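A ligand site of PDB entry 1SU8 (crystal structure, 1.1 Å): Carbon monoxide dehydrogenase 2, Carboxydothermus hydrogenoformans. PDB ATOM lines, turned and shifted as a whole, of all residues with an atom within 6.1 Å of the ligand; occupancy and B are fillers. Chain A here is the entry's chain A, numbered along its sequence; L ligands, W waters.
Water W2 bridges the backbone carbonyl oxygen (O) of Cys 333 and a sulfur (S4) of the ligand.
A sulfur (S5) of the ligand lies close to the backbone carbonyl oxygen (O) of Gly 445, at 3.4 Å.
Cys 294 touches the ligand.
Met 560 touches the ligand (CE to S4, 3.6 Å).
His 561 touches the ligand.
13 residues have an atom within 4 Å of the ligand: His 93, His 261, Cys 294, Cys 295, Ser 312, Cys 333, Gly 445, Cys 446, Cys 476, Cys 526, Met 560, His 561 and Lys 563.
The nearest printed residue that does not touch the ligand is Gly 475 (4.4 Å).
The side-chain sulfur (SG) of Cys 294 lies within hydrogen-bond range of the backbone NH (N) of Ser 312 (3.3 Å).
N of Cys 526 lies close to SG of Cys 295.
The backbone carbonyl oxygen (O) of Gly 445 lies within hydrogen-bond range of the backbone NH (N) of Gly 477 (2.9 Å).
The backbone NH (N) of Cys 476 sits close to the backbone carbonyl oxygen (O) of Gly 445 (3.4 Å).
NZ of Lys 563 lies within hydrogen-bond range of OE1 of Gln 332, at 2.7 Å.
SG of Cys 333 lies close to NZ of Lys 563, 3.2 Å away.
OG of Ser 312 lies within hydrogen-bond range of N of Asn 447, 3.0 Å away.
SG of Cys 446 lies close to N of His 561 (3.3 Å).
An iron atom (FE3) of the ligand is bound by the side-chain sulfur of Cys 446 (2.3 Å).
A ring nitrogen (NE2) of His 93 lies close to a sulfur (S2) of the ligand, 3.6 Å away.
A nickel atom (NI1) of the ligand is bound by the side-chain sulfur (SG) of Cys 526, at 2.3 Å.
The side-chain sulfur of Cys 476 binds an iron atom (FE2) of the ligand (2.3 Å).
The backbone NH (N) of Cys 476 sits close to a sulfur (S5) of the ligand (3.5 Å).
N of Cys 446 sits close to S5 of the ligand (3.6 Å).
SG of Cys 333 is bound to FE4 of the ligand, at 2.2 Å.
A ring nitrogen (NE2) of His 261 is bound to an iron atom (FE1) of the ligand (2.1 Å).
The side-chain amino group (NZ) of Lys 563 lies close to a sulfur (S2) of the ligand, at 3.0 Å.
SG of Cys 295 is bound to FE1 of the ligand (2.3 Å).
The side-chain hydroxyl (OG) of Ser 312 lies close to a sulfur (S4) of the ligand.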
ATOM      1  N   HIS A  93       8.865 -19.943  25.910  1.00  0.00           N
ATOM      2  CA  HIS A  93       7.605 -20.700  25.998  1.00  0.00           C
ATOM      3  C   HIS A  93       7.098 -20.683  27.368  1.00  0.00           C
ATOM      4  O   HIS A  93       5.888 -20.601  27.650  1.00  0.00           O
ATOM      5  CB  HIS A  93       7.872 -22.164  25.626  1.00  0.00           C
ATOM      6  CG  HIS A  93       8.018 -22.330  24.147  1.00  0.00           C
ATOM      7  ND1 HIS A  93       9.012 -23.103  23.667  1.00  0.00           N
ATOM      8  CD2 HIS A  93       7.280 -21.858  23.083  1.00  0.00           C
ATOM      9  CE1 HIS A  93       8.898 -23.105  22.320  1.00  0.00           C
ATOM     10  NE2 HIS A  93       7.856 -22.358  21.949  1.00  0.00           N
ATOM     11  N   GLY A 260       2.561 -12.290  17.340  1.00  0.00           N
ATOM     12  CA  GLY A 260       3.242 -12.660  18.555  1.00  0.00           C
ATOM     13  C   GLY A 260       2.734 -14.030  18.943  1.00  0.00           C
ATOM     14  O   GLY A 260       2.617 -14.893  18.069  1.00  0.00           O
ATOM     15  N   HIS A 261       2.509 -14.197  20.232  1.00  0.00           N
ATOM     16  CA  HIS A 261       2.279 -15.524  20.781  1.00  0.00           C
ATOM     17  C   HIS A 261       1.153 -15.731  21.744  1.00  0.00           C
ATOM     18  O   HIS A 261       0.541 -16.812  21.699  1.00  0.00           O
ATOM     19  CB  HIS A 261       3.573 -15.958  21.625  1.00  0.00           C
ATOM     20  CG  HIS A 261       4.473 -16.425  20.554  1.00  0.00           C
ATOM     21  ND1 HIS A 261       5.188 -15.565  19.714  1.00  0.00           N
ATOM     22  CD2 HIS A 261       4.695 -17.655  20.074  1.00  0.00           C
ATOM     23  CE1 HIS A 261       5.781 -16.288  18.800  1.00  0.00           C
ATOM     24  NE2 HIS A 261       5.513 -17.569  18.986  1.00  0.00           N
ATOM     25  N   CYS A 294       1.886 -15.468  12.716  1.00  0.00           N
ATOM     26  CA  CYS A 294       2.670 -16.254  13.696  1.00  0.00           C
ATOM     27  C   CYS A 294       1.759 -16.945  14.696  1.00  0.00           C
ATOM     28  O   CYS A 294       0.622 -17.278  14.349  1.00  0.00           O
ATOM     29  CB  CYS A 294       3.771 -15.385  14.324  1.00  0.00           C
ATOM     30  SG  CYS A 294       5.177 -15.163  13.174  1.00  0.00           S
ATOM     31  N   CYS A 295       2.275 -17.268  15.880  1.00  0.00           N
ATOM     32  CA  CYS A 295       1.542 -18.210  16.736  1.00  0.00           C
ATOM     33  C   CYS A 295       0.282 -17.620  17.293  1.00  0.00           C
ATOM     34  O   CYS A 295      -0.690 -18.360  17.425  1.00  0.00           O
ATOM     35  CB  CYS A 295       2.452 -18.684  17.900  1.00  0.00           C
ATOM     36  SG  CYS A 295       3.563 -20.010  17.465  1.00  0.00           S
ATOM     37  N   HIS A 311       3.172 -15.658   7.996  1.00  0.00           N
ATOM     38  CA  HIS A 311       3.937 -16.256   9.049  1.00  0.00           C
ATOM     39  C   HIS A 311       5.413 -15.913   8.898  1.00  0.00           C
ATOM     40  O   HIS A 311       5.946 -15.790   7.771  1.00  0.00           O
ATOM     41  CB  HIS A 311       3.869 -17.809   9.000  1.00  0.00           C
ATOM     42  CG  HIS A 311       2.428 -18.299   9.010  1.00  0.00           C
ATOM     43  ND1 HIS A 311       1.713 -18.419   7.838  1.00  0.00           N
ATOM     44  CD2 HIS A 311       1.664 -18.617  10.054  1.00  0.00           C
ATOM     45  CE1 HIS A 311       0.497 -18.823   8.186  1.00  0.00           C
ATOM     46  NE2 HIS A 311       0.429 -18.970   9.517  1.00  0.00           N
ATOM     47  N   SER A 312       6.079 -15.883  10.046  1.00  0.00           N
ATOM     48  CA  SER A 312       7.499 -15.979  10.157  1.00  0.00           C
ATOM     49  C   SER A 312       8.218 -15.001   9.233  1.00  0.00           C
ATOM     50  O   SER A 312       8.032 -13.784   9.291  1.00  0.00           O
ATOM     51  CB  SER A 312       7.880 -17.480   9.922  1.00  0.00           C
ATOM     52  OG  SER A 312       9.219 -17.727  10.323  1.00  0.00           O
ATOM     53  N   VAL A 313       9.087 -15.548   8.419  1.00  0.00           N
ATOM     54  CA  VAL A 313       9.999 -14.713   7.642  1.00  0.00           C
ATOM     55  C   VAL A 313       9.292 -13.708   6.756  1.00  0.00           C
ATOM     56  O   VAL A 313       9.882 -12.654   6.511  1.00  0.00           O
ATOM     57  CB  VAL A 313      10.907 -15.649   6.812  1.00  0.00           C
ATOM     58  CG1 VAL A 313      10.197 -16.330   5.644  1.00  0.00           C
ATOM     59  CG2 VAL A 313      12.118 -14.878   6.291  1.00  0.00           C
ATOM     60  N   GLN A 332       7.705 -12.181  20.969  1.00  0.00           N
ATOM     61  CA  GLN A 332       8.444 -13.225  20.315  1.00  0.00           C
ATOM     62  C   GLN A 332       8.175 -13.282  18.812  1.00  0.00           C
ATOM     63  O   GLN A 332       7.002 -13.254  18.372  1.00  0.00           O
ATOM     64  CB  GLN A 332       8.154 -14.652  20.868  1.00  0.00           C
ATOM     65  CG  GLN A 332       8.390 -14.736  22.398  1.00  0.00           C
ATOM     66  CD  GLN A 332       7.727 -15.987  22.981  1.00  0.00           C
ATOM     67  OE1 GLN A 332       7.326 -16.929  22.263  1.00  0.00           O
ATOM     68  NE2 GLN A 332       7.543 -16.029  24.297  1.00  0.00           N
ATOM     69  N   CYS A 333       9.251 -13.363  18.052  1.00  0.00           N
ATOM     70  CA  CYS A 333       9.215 -13.660  16.613  1.00  0.00           C
ATOM     71  C   CYS A 333       8.708 -12.481  15.777  1.00  0.00           C
ATOM     72  O   CYS A 333       8.426 -12.676  14.572  1.00  0.00           O
ATOM     73  CB  CYS A 333       8.364 -14.926  16.325  1.00  0.00           C
ATOM     74  SG  CYS A 333       9.142 -16.348  17.162  1.00  0.00           S
ATOM     75  N   ALA A 444       7.228 -28.780  12.485  1.00  0.00           N
ATOM     76  CA  ALA A 444       7.182 -27.751  13.506  1.00  0.00           C
ATOM     77  C   ALA A 444       8.171 -26.638  13.155  1.00  0.00           C
ATOM     78  O   ALA A 444       9.046 -26.834  12.317  1.00  0.00           O
ATOM     79  CB  ALA A 444       7.556 -28.370  14.865  1.00  0.00           C
ATOM     80  N   GLY A 445       8.012 -25.544  13.862  1.00  0.00           N
ATOM     81  CA  GLY A 445       9.024 -24.502  13.815  1.00  0.00           C
ATOM     82  C   GLY A 445       8.841 -23.560  12.629  1.00  0.00           C
ATOM     83  O   GLY A 445       7.815 -23.506  11.934  1.00  0.00           O
ATOM     84  N   CYS A 446       9.896 -22.792  12.441  1.00  0.00           N
ATOM     85  CA  CYS A 446       9.909 -21.523  11.726  1.00  0.00           C
ATOM     86  C   CYS A 446      10.113 -21.689  10.240  1.00  0.00           C
ATOM     87  O   CYS A 446      10.367 -22.793   9.740  1.00  0.00           O
ATOM     88  CB  CYS A 446      11.131 -20.717  12.277  1.00  0.00           C
ATOM     89  SG  CYS A 446      11.365 -20.908  14.056  1.00  0.00           S
ATOM     90  N   ASN A 447      10.056 -20.546   9.540  1.00  0.00           N
ATOM     91  CA  ASN A 447      10.826 -20.336   8.313  1.00  0.00           C
ATOM     92  C   ASN A 447      12.146 -19.655   8.689  1.00  0.00           C
ATOM     93  O   ASN A 447      12.264 -19.098   9.775  1.00  0.00           O
ATOM     94  CB  ASN A 447      10.098 -19.422   7.320  1.00  0.00           C
ATOM     95  CG  ASN A 447       8.762 -19.965   6.808  1.00  0.00           C
ATOM     96  OD1 ASN A 447       8.691 -21.095   6.232  1.00  0.00           O
ATOM     97  ND2 ASN A 447       7.753 -19.175   6.924  1.00  0.00           N
ATOM     98  N   THR A 474       2.417 -27.797  13.317  1.00  0.00           N
ATOM     99  CA  THR A 474       2.162 -26.689  14.240  1.00  0.00           C
ATOM    100  C   THR A 474       2.963 -25.473  13.801  1.00  0.00           C
ATOM    101  O   THR A 474       3.884 -25.543  12.982  1.00  0.00           O
ATOM    102  CB  THR A 474       2.615 -27.058  15.677  1.00  0.00           C
ATOM    103  OG1 THR A 474       4.032 -27.298  15.590  1.00  0.00           O
ATOM    104  CG2 THR A 474       1.890 -28.284  16.215  1.00  0.00           C
ATOM    105  N   GLY A 475       2.629 -24.346  14.439  1.00  0.00           N
ATOM    106  CA  GLY A 475       3.381 -23.109  14.269  1.00  0.00           C
ATOM    107  C   GLY A 475       3.541 -22.717  12.853  1.00  0.00           C
ATOM    108  O   GLY A 475       2.607 -22.771  12.046  1.00  0.00           O
ATOM    109  N   CYS A 476       4.730 -22.232  12.517  1.00  0.00           N
ATOM    110  CA  CYS A 476       4.926 -21.739  11.156  1.00  0.00           C
ATOM    111  C   CYS A 476       5.180 -22.881  10.184  1.00  0.00           C
ATOM    112  O   CYS A 476       5.120 -22.677   8.974  1.00  0.00           O
ATOM    113  CB  CYS A 476       6.028 -20.670  11.216  1.00  0.00           C
ATOM    114  SG  CYS A 476       5.453 -19.197  12.195  1.00  0.00           S
ATOM    115  N   GLY A 477       5.332 -24.115  10.662  1.00  0.00           N
ATOM    116  CA  GLY A 477       5.309 -25.270   9.776  1.00  0.00           C
ATOM    117  C   GLY A 477       3.869 -25.464   9.282  1.00  0.00           C
ATOM    118  O   GLY A 477       3.619 -25.678   8.073  1.00  0.00           O
ATOM    119  N   SER A 525      -0.546 -23.844  17.559  1.00  0.00           N
ATOM    120  CA  SER A 525       0.646 -22.992  17.716  1.00  0.00           C
ATOM    121  C   SER A 525       1.858 -23.804  18.156  1.00  0.00           C
ATOM    122  O   SER A 525       1.781 -25.033  18.341  1.00  0.00           O
ATOM    123  CB  SER A 525       0.333 -21.956  18.822  1.00  0.00           C
ATOM    124  OG  SER A 525       0.152 -22.721  20.006  1.00  0.00           O
ATOM    125  N   CYS A 526       2.993 -23.125  18.327  1.00  0.00           N
ATOM    126  CA  CYS A 526       4.199 -23.882  18.724  1.00  0.00           C
ATOM    127  C   CYS A 526       4.072 -24.451  20.135  1.00  0.00           C
ATOM    128  O   CYS A 526       4.526 -25.560  20.351  1.00  0.00           O
ATOM    129  CB  CYS A 526       5.391 -22.929  18.669  1.00  0.00           C
ATOM    130  SG  CYS A 526       5.801 -22.495  16.955  1.00  0.00           S
ATOM    131  N   VAL A 527       3.434 -23.735  21.090  1.00  0.00           N
ATOM    132  CA  VAL A 527       3.269 -24.441  22.381  1.00  0.00           C
ATOM    133  C   VAL A 527       2.426 -25.691  22.196  1.00  0.00           C
ATOM    134  O   VAL A 527       2.594 -26.661  22.900  1.00  0.00           O
ATOM    135  CB  VAL A 527       2.701 -23.536  23.495  1.00  0.00           C
ATOM    136  CG1 VAL A 527       3.713 -22.456  23.920  1.00  0.00           C
ATOM    137  CG2 VAL A 527       1.363 -22.861  23.126  1.00  0.00           C
ATOM    138  N   MET A 560      14.464 -21.551  13.002  1.00  0.00           N
ATOM    139  CA  MET A 560      15.089 -20.227  13.198  1.00  0.00           C
ATOM    140  C   MET A 560      15.292 -19.954  14.689  1.00  0.00           C
ATOM    141  O   MET A 560      16.382 -19.649  15.122  1.00  0.00           O
ATOM    142  CB  MET A 560      14.237 -19.154  12.488  1.00  0.00           C
ATOM    143  CG  MET A 560      14.737 -17.750  12.681  1.00  0.00           C
ATOM    144  SD  MET A 560      14.052 -16.833  14.099  1.00  0.00           S
ATOM    145  CE  MET A 560      12.269 -16.894  13.755  1.00  0.00           C
ATOM    146  N   HIS A 561      14.201 -19.947  15.445  1.00  0.00           N
ATOM    147  CA  HIS A 561      14.260 -19.336  16.786  1.00  0.00           C
ATOM    148  C   HIS A 561      14.915 -20.255  17.784  1.00  0.00           C
ATOM    149  O   HIS A 561      14.906 -21.494  17.641  1.00  0.00           O
ATOM    150  CB  HIS A 561      12.821 -19.000  17.210  1.00  0.00           C
ATOM    151  CG  HIS A 561      12.711 -17.978  18.282  1.00  0.00           C
ATOM    152  ND1 HIS A 561      12.929 -18.279  19.610  1.00  0.00           N
ATOM    153  CD2 HIS A 561      12.456 -16.670  18.161  1.00  0.00           C
ATOM    154  CE1 HIS A 561      12.775 -17.156  20.276  1.00  0.00           C
ATOM    155  NE2 HIS A 561      12.464 -16.152  19.437  1.00  0.00           N
ATOM    156  N   LYS A 563      13.515 -20.944  20.415  1.00  0.00           N
ATOM    157  CA  LYS A 563      12.379 -21.839  20.795  1.00  0.00           C
ATOM    158  C   LYS A 563      12.357 -23.097  19.935  1.00  0.00           C
ATOM    159  O   LYS A 563      11.995 -24.160  20.431  1.00  0.00           O
ATOM    160  CB  LYS A 563      11.083 -21.072  20.642  1.00  0.00           C
ATOM    161  CG  LYS A 563      10.881 -20.007  21.768  1.00  0.00           C
ATOM    162  CD  LYS A 563       9.562 -19.258  21.593  1.00  0.00           C
ATOM    163  CE  LYS A 563       9.687 -18.303  20.400  1.00  0.00           C
ATOM    164  NZ  LYS A 563       8.344 -17.841  19.932  1.00  0.00           N
ATOM    165  N   ALA A 564      12.683 -23.006  18.630  1.00  0.00           N
ATOM    166  CA  ALA A 564      12.649 -24.177  17.784  1.00  0.00           C
ATOM    167  C   ALA A 564      13.771 -25.121  18.143  1.00  0.00           C
ATOM    168  O   ALA A 564      13.598 -26.331  18.030  1.00  0.00           O
ATOM    169  CB  ALA A 564      12.716 -23.726  16.319  1.00  0.00           C
ATOM    170  N   ILE A 567      12.452 -26.964  21.147  1.00  0.00           N
ATOM    171  CA  ILE A 567      11.440 -27.980  20.779  1.00  0.00           C
ATOM    172  C   ILE A 567      12.119 -29.170  20.130  1.00  0.00           C
ATOM    173  O   ILE A 567      11.852 -30.328  20.441  1.00  0.00           O
ATOM    174  CB  ILE A 567      10.413 -27.332  19.841  1.00  0.00           C
ATOM    175  CG1 ILE A 567       9.475 -26.403  20.631  1.00  0.00           C
ATOM    176  CG2 ILE A 567       9.644 -28.467  19.087  1.00  0.00           C
ATOM    177  CD1 ILE A 567       8.752 -25.373  19.751  1.00  0.00           C
HETATM  178 NI1  LIG L   1       7.619 -21.167  16.891  1.00  0.00          NI
HETATM  179 FE1  LIG L   1       5.754 -19.208  17.703  1.00  0.00          FE
HETATM  180 FE2  LIG L   1       6.888 -19.127  13.984  1.00  0.00          FE
HETATM  181 FE3  LIG L   1       9.297 -20.122  14.793  1.00  0.00          FE
HETATM  182 FE4  LIG L   1       8.323 -18.041  15.958  1.00  0.00          FE
HETATM  183  S1  LIG L   1       6.046 -17.953  15.762  1.00  0.00           S
HETATM  184  S2  LIG L   1       7.143 -20.481  19.014  1.00  0.00           S
HETATM  185  S3  LIG L   1       9.404 -19.797  16.970  1.00  0.00           S
HETATM  186  S4  LIG L   1       8.923 -18.125  13.671  1.00  0.00           S
HETATM  187  S5  LIG L   1       7.404 -21.352  14.596  1.00  0.00           S
HETATM  188  O   HOH W   1       8.949 -22.651  18.007  1.00  0.00           O
HETATM  189  O   HOH W   2       9.281 -14.728  12.933  1.00  0.00           O
